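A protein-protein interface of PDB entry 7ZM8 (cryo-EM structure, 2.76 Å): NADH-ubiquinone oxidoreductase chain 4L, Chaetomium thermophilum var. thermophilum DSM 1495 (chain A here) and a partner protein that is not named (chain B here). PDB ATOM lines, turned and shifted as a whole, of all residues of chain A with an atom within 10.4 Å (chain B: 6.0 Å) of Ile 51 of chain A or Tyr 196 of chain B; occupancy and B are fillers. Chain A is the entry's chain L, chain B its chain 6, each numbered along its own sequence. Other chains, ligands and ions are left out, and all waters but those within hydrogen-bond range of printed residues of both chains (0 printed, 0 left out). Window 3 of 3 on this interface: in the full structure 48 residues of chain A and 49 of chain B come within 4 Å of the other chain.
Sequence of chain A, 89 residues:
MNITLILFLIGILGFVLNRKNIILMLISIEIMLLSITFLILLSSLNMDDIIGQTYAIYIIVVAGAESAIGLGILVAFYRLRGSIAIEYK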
ATOM      1  N   THR A  37      -8.323 -27.087   5.513  1.00  0.00           N
ATOM      2  CA  THR A  37      -7.856 -26.521   6.806  1.00  0.00           C
ATOM      3  C   THR A  37      -6.383 -26.867   7.047  1.00  0.00           C
ATOM      4  O   THR A  37      -5.657 -25.974   7.493  1.00  0.00           O
ATOM      5  CB  THR A  37      -8.808 -26.853   7.964  1.00  0.00           C
ATOM      6  OG1 THR A  37      -8.299 -26.251   9.153  1.00  0.00           O
ATOM      7  CG2 THR A  37      -8.992 -28.334   8.197  1.00  0.00           C
ATOM      8  N   ILE A  40      -4.199 -24.571   4.904  1.00  0.00           N
ATOM      9  CA  ILE A  40      -4.129 -23.219   5.526  1.00  0.00           C
ATOM     10  C   ILE A  40      -3.205 -23.280   6.739  1.00  0.00           C
ATOM     11  O   ILE A  40      -2.385 -22.374   6.869  1.00  0.00           O
ATOM     12  CB  ILE A  40      -5.543 -22.718   5.897  1.00  0.00           C
ATOM     13  CG1 ILE A  40      -6.411 -22.505   4.659  1.00  0.00           C
ATOM     14  CG2 ILE A  40      -5.485 -21.462   6.752  1.00  0.00           C
ATOM     15  CD1 ILE A  40      -7.863 -22.773   4.904  1.00  0.00           C
ATOM     16  N   LEU A  41      -3.313 -24.322   7.563  1.00  0.00           N
ATOM     17  CA  LEU A  41      -2.506 -24.463   8.800  1.00  0.00           C
ATOM     18  C   LEU A  41      -1.011 -24.613   8.521  1.00  0.00           C
ATOM     19  O   LEU A  41      -0.221 -24.078   9.302  1.00  0.00           O
ATOM     20  CB  LEU A  41      -3.058 -25.619   9.629  1.00  0.00           C
ATOM     21  CG  LEU A  41      -4.204 -25.253  10.565  1.00  0.00           C
ATOM     22  CD1 LEU A  41      -4.543 -26.421  11.468  1.00  0.00           C
ATOM     23  CD2 LEU A  41      -3.844 -24.031  11.394  1.00  0.00           C
ATOM     24  N   LEU A  42      -0.636 -25.319   7.465  1.00  0.00           N
ATOM     25  CA  LEU A  42       0.791 -25.583   7.136  1.00  0.00           C
ATOM     26  C   LEU A  42       1.358 -24.347   6.448  1.00  0.00           C
ATOM     27  O   LEU A  42       2.516 -24.032   6.704  1.00  0.00           O
ATOM     28  CB  LEU A  42       0.915 -26.814   6.234  1.00  0.00           C
ATOM     29  CG  LEU A  42       0.566 -28.163   6.847  1.00  0.00           C
ATOM     30  CD1 LEU A  42       1.129 -29.288   5.998  1.00  0.00           C
ATOM     31  CD2 LEU A  42       1.095 -28.257   8.258  1.00  0.00           C
ATOM     32  N   SER A  43       0.561 -23.671   5.629  1.00  0.00           N
ATOM     33  CA  SER A  43       1.026 -22.420   5.053  1.00  0.00           C
ATOM     34  C   SER A  43       1.110 -21.314   6.088  1.00  0.00           C
ATOM     35  O   SER A  43       1.801 -20.319   5.862  1.00  0.00           O
ATOM     36  CB  SER A  43       0.103 -22.001   3.911  1.00  0.00           C
ATOM     37  OG  SER A  43      -0.052 -23.054   2.978  1.00  0.00           O
ATOM     38  N   SER A  44       0.358 -21.410   7.167  1.00  0.00           N
ATOM     39  CA  SER A  44       0.384 -20.405   8.261  1.00  0.00           C
ATOM     40  C   SER A  44       1.708 -20.500   9.017  1.00  0.00           C
ATOM     41  O   SER A  44       2.315 -19.455   9.243  1.00  0.00           O
ATOM     42  CB  SER A  44      -0.803 -20.578   9.135  1.00  0.00           C
ATOM     43  OG  SER A  44      -1.981 -20.430   8.369  1.00  0.00           O
ATOM     44  N   LEU A  45       2.132 -21.710   9.377  1.00  0.00           N
ATOM     45  CA  LEU A  45       3.450 -21.930  10.021  1.00  0.00           C
ATOM     46  C   LEU A  45       4.571 -21.458   9.082  1.00  0.00           C
ATOM     47  O   LEU A  45       5.596 -20.998   9.597  1.00  0.00           O
ATOM     48  CB  LEU A  45       3.558 -23.423  10.345  1.00  0.00           C
ATOM     49  CG  LEU A  45       4.722 -23.854  11.229  1.00  0.00           C
ATOM     50  CD1 LEU A  45       4.540 -23.331  12.642  1.00  0.00           C
ATOM     51  CD2 LEU A  45       4.833 -25.368  11.238  1.00  0.00           C
ATOM     52  N   MET A  47       4.552 -18.892   7.070  1.00  0.00           N
ATOM     53  CA  MET A  47       4.543 -17.415   6.899  1.00  0.00           C
ATOM     54  C   MET A  47       4.483 -16.699   8.245  1.00  0.00           C
ATOM     55  O   MET A  47       4.355 -15.472   8.217  1.00  0.00           O
ATOM     56  CB  MET A  47       3.346 -17.000   6.044  1.00  0.00           C
ATOM     57  CG  MET A  47       3.307 -17.649   4.674  1.00  0.00           C
ATOM     58  SD  MET A  47       1.915 -17.092   3.647  1.00  0.00           S
ATOM     59  CE  MET A  47       0.541 -17.293   4.777  1.00  0.00           C
ATOM     60  N   ASP A  48       4.607 -17.414   9.361  1.00  0.00           N
ATOM     61  CA  ASP A  48       4.552 -16.839  10.736  1.00  0.00           C
ATOM     62  C   ASP A  48       3.281 -16.024  10.934  1.00  0.00           C
ATOM     63  O   ASP A  48       3.380 -14.907  11.442  1.00  0.00           O
ATOM     64  CB  ASP A  48       5.793 -16.023  11.093  1.00  0.00           C
ATOM     65  CG  ASP A  48       5.948 -15.766  12.582  1.00  0.00           C
ATOM     66  OD1 ASP A  48       5.967 -16.750  13.343  1.00  0.00           O
ATOM     67  OD2 ASP A  48       6.033 -14.580  12.969  1.00  0.00           O
ATOM     68  N   ASP A  49       2.137 -16.563  10.542  1.00  0.00           N
ATOM     69  CA  ASP A  49       0.880 -15.779  10.603  1.00  0.00           C
ATOM     70  C   ASP A  49      -0.122 -16.507  11.494  1.00  0.00           C
ATOM     71  O   ASP A  49      -0.500 -17.632  11.165  1.00  0.00           O
ATOM     72  CB  ASP A  49       0.354 -15.506   9.195  1.00  0.00           C
ATOM     73  CG  ASP A  49      -0.362 -14.175   9.063  1.00  0.00           C
ATOM     74  OD1 ASP A  49      -0.431 -13.450  10.074  1.00  0.00           O
ATOM     75  OD2 ASP A  49      -0.846 -13.875   7.951  1.00  0.00           O
ATOM     76  N   ILE A  50      -0.538 -15.873  12.578  1.00  0.00           N
ATOM     77  CA  ILE A  50      -1.521 -16.479  13.471  1.00  0.00           C
ATOM     78  C   ILE A  50      -2.934 -16.376  12.926  1.00  0.00           C
ATOM     79  O   ILE A  50      -3.840 -17.023  13.461  1.00  0.00           O
ATOM     80  CB  ILE A  50      -1.435 -15.835  14.869  1.00  0.00           C
ATOM     81  CG1 ILE A  50      -1.943 -16.797  15.948  1.00  0.00           C
ATOM     82  CG2 ILE A  50      -2.216 -14.538  14.910  1.00  0.00           C
ATOM     83  CD1 ILE A  50      -1.014 -17.947  16.242  1.00  0.00           C
ATOM     84  N   ILE A  51      -3.149 -15.591  11.870  1.00  0.00           N
ATOM     85  CA  ILE A  51      -4.497 -15.413  11.343  1.00  0.00           C
ATOM     86  C   ILE A  51      -4.936 -16.648  10.574  1.00  0.00           C
ATOM     87  O   ILE A  51      -6.134 -16.918  10.438  1.00  0.00           O
ATOM     88  CB  ILE A  51      -4.570 -14.145  10.475  1.00  0.00           C
ATOM     89  CG1 ILE A  51      -6.017 -13.697  10.306  1.00  0.00           C
ATOM     90  CG2 ILE A  51      -3.955 -14.393   9.117  1.00  0.00           C
ATOM     91  CD1 ILE A  51      -6.152 -12.325   9.737  1.00  0.00           C
ATOM     92  N   GLY A  52      -3.977 -17.414  10.051  1.00  0.00           N
ATOM     93  CA  GLY A  52      -4.316 -18.685   9.441  1.00  0.00           C
ATOM     94  C   GLY A  52      -4.839 -19.685  10.451  1.00  0.00           C
ATOM     95  O   GLY A  52      -5.735 -20.473  10.153  1.00  0.00           O
ATOM     96  N   GLN A  53      -4.278 -19.669  11.658  1.00  0.00           N
ATOM     97  CA  GLN A  53      -4.771 -20.536  12.718  1.00  0.00           C
ATOM     98  C   GLN A  53      -6.183 -20.153  13.123  1.00  0.00           C
ATOM     99  O   GLN A  53      -6.979 -21.013  13.509  1.00  0.00           O
ATOM    100  CB  GLN A  53      -3.835 -20.461  13.918  1.00  0.00           C
ATOM    101  CG  GLN A  53      -2.425 -20.870  13.619  1.00  0.00           C
ATOM    102  CD  GLN A  53      -1.756 -21.515  14.799  1.00  0.00           C
ATOM    103  OE1 GLN A  53      -2.419 -22.054  15.676  1.00  0.00           O
ATOM    104  NE2 GLN A  53      -0.437 -21.457  14.836  1.00  0.00           N
ATOM    105  N   THR A  54      -6.500 -18.863  13.068  1.00  0.00           N
ATOM    106  CA  THR A  54      -7.839 -18.407  13.411  1.00  0.00           C
ATOM    107  C   THR A  54      -8.844 -18.827  12.349  1.00  0.00           C
ATOM    108  O   THR A  54      -9.947 -19.281  12.666  1.00  0.00           O
ATOM    109  CB  THR A  54      -7.829 -16.892  13.573  1.00  0.00           C
ATOM    110  OG1 THR A  54      -6.912 -16.539  14.611  1.00  0.00           O
ATOM    111  CG2 THR A  54      -9.209 -16.393  13.944  1.00  0.00           C
ATOM    112  N   TYR A  55      -8.467 -18.688  11.078  1.00  0.00           N
ATOM    113  CA  TYR A  55      -9.321 -19.124   9.982  1.00  0.00           C
ATOM    114  C   TYR A  55      -9.531 -20.631  10.002  1.00  0.00           C
ATOM    115  O   TYR A  55     -10.624 -21.113   9.693  1.00  0.00           O
ATOM    116  CB  TYR A  55      -8.732 -18.611   8.667  1.00  0.00           C
ATOM    117  CG  TYR A  55      -9.497 -18.932   7.408  1.00  0.00           C
ATOM    118  CD1 TYR A  55     -10.666 -18.271   7.116  1.00  0.00           C
ATOM    119  CD2 TYR A  55      -8.943 -19.705   6.411  1.00  0.00           C
ATOM    120  CE1 TYR A  55     -11.360 -18.489   5.956  1.00  0.00           C
ATOM    121  CE2 TYR A  55      -9.618 -19.915   5.219  1.00  0.00           C
ATOM    122  CZ  TYR A  55     -10.830 -19.304   5.004  1.00  0.00           C
ATOM    123  OH  TYR A  55     -11.524 -19.497   3.830  1.00  0.00           O
ATOM    124  N   ALA A  56      -8.510 -21.391  10.390  1.00  0.00           N
ATOM    125  CA  ALA A  56      -8.691 -22.828  10.562  1.00  0.00           C
ATOM    126  C   ALA A  56      -9.709 -23.131  11.652  1.00  0.00           C
ATOM    127  O   ALA A  56     -10.537 -24.033  11.502  1.00  0.00           O
ATOM    128  CB  ALA A  56      -7.355 -23.491  10.880  1.00  0.00           C
ATOM    129  N   ILE A  57      -9.662 -22.385  12.758  1.00  0.00           N
ATOM    130  CA  ILE A  57     -10.587 -22.617  13.864  1.00  0.00           C
ATOM    131  C   ILE A  57     -12.026 -22.379  13.423  1.00  0.00           C
ATOM    132  O   ILE A  57     -12.926 -23.161  13.741  1.00  0.00           O
ATOM    133  CB  ILE A  57     -10.208 -21.733  15.066  1.00  0.00           C
ATOM    134  CG1 ILE A  57      -8.948 -22.264  15.749  1.00  0.00           C
ATOM    135  CG2 ILE A  57     -11.352 -21.652  16.062  1.00  0.00           C
ATOM    136  CD1 ILE A  57      -9.098 -23.657  16.314  1.00  0.00           C
ATOM    137  N   TYR A  58     -12.266 -21.296  12.687  1.00  0.00           N
ATOM    138  CA  TYR A  58     -13.624 -20.999  12.254  1.00  0.00           C
ATOM    139  C   TYR A  58     -14.108 -21.983  11.201  1.00  0.00           C
ATOM    140  O   TYR A  58     -15.316 -22.217  11.089  1.00  0.00           O
ATOM    141  CB  TYR A  58     -13.705 -19.569  11.734  1.00  0.00           C
ATOM    142  CG  TYR A  58     -13.695 -18.545  12.840  1.00  0.00           C
ATOM    143  CD1 TYR A  58     -14.682 -18.539  13.811  1.00  0.00           C
ATOM    144  CD2 TYR A  58     -12.700 -17.594  12.918  1.00  0.00           C
ATOM    145  CE1 TYR A  58     -14.676 -17.613  14.820  1.00  0.00           C
ATOM    146  CE2 TYR A  58     -12.687 -16.667  13.926  1.00  0.00           C
ATOM    147  CZ  TYR A  58     -13.674 -16.679  14.872  1.00  0.00           C
ATOM    148  OH  TYR A  58     -13.651 -15.744  15.875  1.00  0.00           O
ATOM    149  N   ILE A  59     -13.181 -22.605  10.469  1.00  0.00           N
ATOM    150  CA  ILE A  59     -13.593 -23.620   9.464  1.00  0.00           C
ATOM    151  C   ILE A  59     -14.004 -24.886  10.207  1.00  0.00           C
ATOM    152  O   ILE A  59     -14.956 -25.514   9.766  1.00  0.00           O
ATOM    153  CB  ILE A  59     -12.453 -23.874   8.458  1.00  0.00           C
ATOM    154  CG1 ILE A  59     -12.227 -22.691   7.519  1.00  0.00           C
ATOM    155  CG2 ILE A  59     -12.682 -25.154   7.670  1.00  0.00           C
ATOM    156  CD1 ILE A  59     -10.988 -22.848   6.686  1.00  0.00           C
ATOM    157  N   ILE B 191      -6.168 -11.547  19.667  1.00  0.00           N
ATOM    158  CA  ILE B 191      -6.806 -10.859  18.505  1.00  0.00           C
ATOM    159  C   ILE B 191      -8.225 -11.377  18.243  1.00  0.00           C
ATOM    160  O   ILE B 191      -8.971 -10.669  17.552  1.00  0.00           O
ATOM    161  CB  ILE B 191      -5.887 -11.006  17.268  1.00  0.00           C
ATOM    162  CG1 ILE B 191      -5.781 -12.462  16.812  1.00  0.00           C
ATOM    163  CG2 ILE B 191      -4.522 -10.398  17.527  1.00  0.00           C
ATOM    164  CD1 ILE B 191      -5.559 -12.626  15.334  1.00  0.00           C
ATOM    165  N   MET B 192      -8.601 -12.530  18.803  1.00  0.00           N
ATOM    166  CA  MET B 192      -9.858 -13.190  18.475  1.00  0.00           C
ATOM    167  C   MET B 192     -11.067 -12.408  18.975  1.00  0.00           C
ATOM    168  O   MET B 192     -12.152 -12.504  18.392  1.00  0.00           O
ATOM    169  CB  MET B 192      -9.836 -14.596  19.066  1.00  0.00           C
ATOM    170  CG  MET B 192     -11.129 -15.350  19.072  1.00  0.00           C
ATOM    171  SD  MET B 192     -10.854 -17.022  19.659  1.00  0.00           S
ATOM    172  CE  MET B 192     -12.507 -17.661  19.500  1.00  0.00           C
ATOM    173  N   TYR B 193     -10.914 -11.669  20.075  1.00  0.00           N
ATOM    174  CA  TYR B 193     -12.082 -11.014  20.701  1.00  0.00           C
ATOM    175  C   TYR B 193     -12.049  -9.501  20.545  1.00  0.00           C
ATOM    176  O   TYR B 193     -12.931  -8.841  21.073  1.00  0.00           O
ATOM    177  CB  TYR B 193     -12.173 -11.409  22.173  1.00  0.00           C
ATOM    178  CG  TYR B 193     -12.070 -12.878  22.451  1.00  0.00           C
ATOM    179  CD1 TYR B 193     -13.194 -13.683  22.443  1.00  0.00           C
ATOM    180  CD2 TYR B 193     -10.848 -13.454  22.725  1.00  0.00           C
ATOM    181  CE1 TYR B 193     -13.100 -15.038  22.695  1.00  0.00           C
ATOM    182  CE2 TYR B 193     -10.733 -14.807  22.966  1.00  0.00           C
ATOM    183  CZ  TYR B 193     -11.864 -15.596  22.960  1.00  0.00           C
ATOM    184  OH  TYR B 193     -11.747 -16.920  23.228  1.00  0.00           O
ATOM    185  N   THR B 194     -11.073  -8.978  19.802  1.00  0.00           N
ATOM    186  CA  THR B 194     -10.936  -7.506  19.639  1.00  0.00           C
ATOM    187  C   THR B 194     -10.860  -7.133  18.161  1.00  0.00           C
ATOM    188  O   THR B 194     -11.884  -6.707  17.626  1.00  0.00           O
ATOM    189  CB  THR B 194      -9.747  -6.973  20.451  1.00  0.00           C
ATOM    190  OG1 THR B 194      -8.625  -7.821  20.211  1.00  0.00           O
ATOM    191  CG2 THR B 194     -10.025  -6.910  21.935  1.00  0.00           C
ATOM    192  N   ASN B 195      -9.700  -7.308  17.531  1.00  0.00           N
ATOM    193  CA  ASN B 195      -9.468  -6.884  16.124  1.00  0.00           C
ATOM    194  C   ASN B 195     -10.369  -7.611  15.126  1.00  0.00           C
ATOM    195  O   ASN B 195     -10.878  -6.943  14.216  1.00  0.00           O
ATOM    196  CB  ASN B 195      -8.012  -7.143  15.729  1.00  0.00           C
ATOM    197  CG  ASN B 195      -6.980  -6.435  16.578  1.00  0.00           C
ATOM    198  OD1 ASN B 195      -6.261  -5.571  16.084  1.00  0.00           O
ATOM    199  ND2 ASN B 195      -6.871  -6.809  17.842  1.00  0.00           N
ATOM    200  N   TYR B 196     -10.568  -8.915  15.293  1.00  0.00           N
ATOM    201  CA  TYR B 196     -11.336  -9.729  14.314  1.00  0.00           C
ATOM    202  C   TYR B 196     -12.614 -10.232  14.988  1.00  0.00           C
ATOM    203  O   TYR B 196     -13.055 -11.338  14.645  1.00  0.00           O
ATOM    204  CB  TYR B 196     -10.456 -10.835  13.733  1.00  0.00           C
ATOM    205  CG  TYR B 196      -9.199 -10.358  13.051  1.00  0.00           C
ATOM    206  CD1 TYR B 196      -8.002 -10.265  13.739  1.00  0.00           C
ATOM    207  CD2 TYR B 196      -9.209  -9.989  11.719  1.00  0.00           C
ATOM    208  CE1 TYR B 196      -6.847  -9.821  13.122  1.00  0.00           C
ATOM    209  CE2 TYR B 196      -8.063  -9.544  11.085  1.00  0.00           C
ATOM    210  CZ  TYR B 196      -6.876  -9.459  11.788  1.00  0.00           C
ATOM    211  OH  TYR B 196      -5.744  -9.022  11.167  1.00  0.00           O
ATOM    212  N   ASN B 197     -13.198  -9.442  15.893  1.00  0.00           N
ATOM    213  CA  ASN B 197     -14.390  -9.868  16.681  1.00  0.00           C
ATOM    214  C   ASN B 197     -15.627 -10.111  15.806  1.00  0.00           C
ATOM    215  O   ASN B 197     -16.539 -10.792  16.281  1.00  0.00           O
ATOM    216  CB  ASN B 197     -14.623  -8.976  17.909  1.00  0.00           C
ATOM    217  CG  ASN B 197     -14.978  -7.539  17.598  1.00  0.00           C
ATOM    218  OD1 ASN B 197     -15.079  -7.146  16.440  1.00  0.00           O
ATOM    219  ND2 ASN B 197     -15.171  -6.744  18.636  1.00  0.00           N
ATOM    220  N   VAL B 198     -15.683  -9.527  14.611  1.00  0.00           N
ATOM    221  CA  VAL B 198     -16.838  -9.711  13.676  1.00  0.00           C
ATOM    222  C   VAL B 198     -16.946 -11.188  13.276  1.00  0.00           C
ATOM    223  O   VAL B 198     -18.078 -11.673  13.138  1.00  0.00           O
ATOM    224  CB  VAL B 198     -16.769  -8.740  12.477  1.00  0.00           C
ATOM    225  CG1 VAL B 198     -17.211  -9.362  11.161  1.00  0.00           C
ATOM    226  CG2 VAL B 198     -17.541  -7.463  12.757  1.00  0.00           C
ATOM    227  N   TRP B 199     -15.817 -11.874  13.107  1.00  0.00           N
ATOM    228  CA  TRP B 199     -15.834 -13.329  12.788  1.00  0.00           C
ATOM    229  C   TRP B 199     -16.484 -14.116  13.930  1.00  0.00           C
ATOM    230  O   TRP B 199     -17.219 -15.059  13.630  1.00  0.00           O
ATOM    231  CB  TRP B 199     -14.428 -13.850  12.488  1.00  0.00           C
ATOM    232  CG  TRP B 199     -13.755 -13.220  11.310  1.00  0.00           C
ATOM    233  CD1 TRP B 199     -14.337 -12.519  10.298  1.00  0.00           C
ATOM    234  CD2 TRP B 199     -12.348 -13.255  11.018  1.00  0.00           C
ATOM    235  NE1 TRP B 199     -13.390 -12.107   9.401  1.00  0.00           N
ATOM    236  CE2 TRP B 199     -12.160 -12.542   9.816  1.00  0.00           C
ATOM    237  CE3 TRP B 199     -11.236 -13.818  11.651  1.00  0.00           C
ATOM    238  CZ2 TRP B 199     -10.903 -12.373   9.242  1.00  0.00           C
ATOM    239  CZ3 TRP B 199      -9.995 -13.655  11.081  1.00  0.00           C
ATOM    240  CH2 TRP B 199      -9.835 -12.945   9.891  1.00  0.00           C
ATOM    241  N   LEU B 200     -16.206 -13.751  15.182  1.00  0.00           N
ATOM    242  CA  LEU B 200     -16.813 -14.422  16.357  1.00  0.00           C
ATOM    243  C   LEU B 200     -18.322 -14.193  16.337  1.00  0.00           C
ATOM    244  O   LEU B 200     -19.061 -15.138  16.609  1.00  0.00           O
ATOM    245  CB  LEU B 200     -16.194 -13.806  17.615  1.00  0.00           C
ATOM    246  CG  LEU B 200     -16.496 -14.510  18.935  1.00  0.00           C
ATOM    247  CD1 LEU B 200     -15.865 -15.893  18.971  1.00  0.00           C
ATOM    248  CD2 LEU B 200     -16.002 -13.671  20.099  1.00  0.00           C
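Of chain B, only Tyr 196 (3.6 Å) and Trp 199 (3.7 Å) come within 4 Å of Ile 51 of chain A. Tyr 196 of chain B touches one residue of chain A. Of chain A, only Ile 50 (3.9 Å) comes within 4 Å of Ile 191 of chain B. No residue of chain A comes within 4 Å of Asn 197 of chain B. Val 198 of chain B touches none of the printed residues of chain A. Of the printed residues of chain B, Thr 54 of chain A touches Trp 199 (3.9997 Å). Printed residues of chain B within 4 Å of Ile 50 of chain A: Ile 191 (3.9 Å). The nearest residue of chain B that does not touch Ile 51 of chain A is Ile 191 of chain B (5.0 Å). The nearest residue of chain A that does not touch Tyr 196 of chain B is Tyr 58 of chain A (4.6 Å). The nearest printed residue of chain B that does not touch Thr 54 of chain A is Ile 191 of chain B (4.2 Å).
The backbone NH (N) of Leu 200 of chain B lies within hydrogen-bond range of the side-chain hydroxyl (OH) of Tyr 58 of chain A (3.3 Å).
O of Ile 50 of chain A lies within hydrogen-bond range of OG1 of Thr 54 of chain A, at 3.3 Å. O of Ile 191 of chain B lies within hydrogen-bond range of N of Tyr 196 of chain B.
Hydrophobic or aromatic side chains of chain A that line the printed part of chain B: Ile 50, Ile 51 and Tyr 58. Of the 10 printed residues of chain B, 4 touch a printed residue of chain A. Among the printed residues, 6 pairs touch across the chains.
CG2 of Ile 50 of chain A touches CD1 of Ile 191 of chain B, 3.9 Å away. Ile 51 of chain A touches Tyr 196 of chain B (CD1 to CZ, 3.6 Å). Trp 199 of chain B touches Ile 51 of chain A. Thr 54 of chain A touches Trp 199 of chain B (CG2 to CE3, 3.9997 Å). Trp 199 of chain B touches Tyr 58 of chain A (CB to CE2, 3.6 Å).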
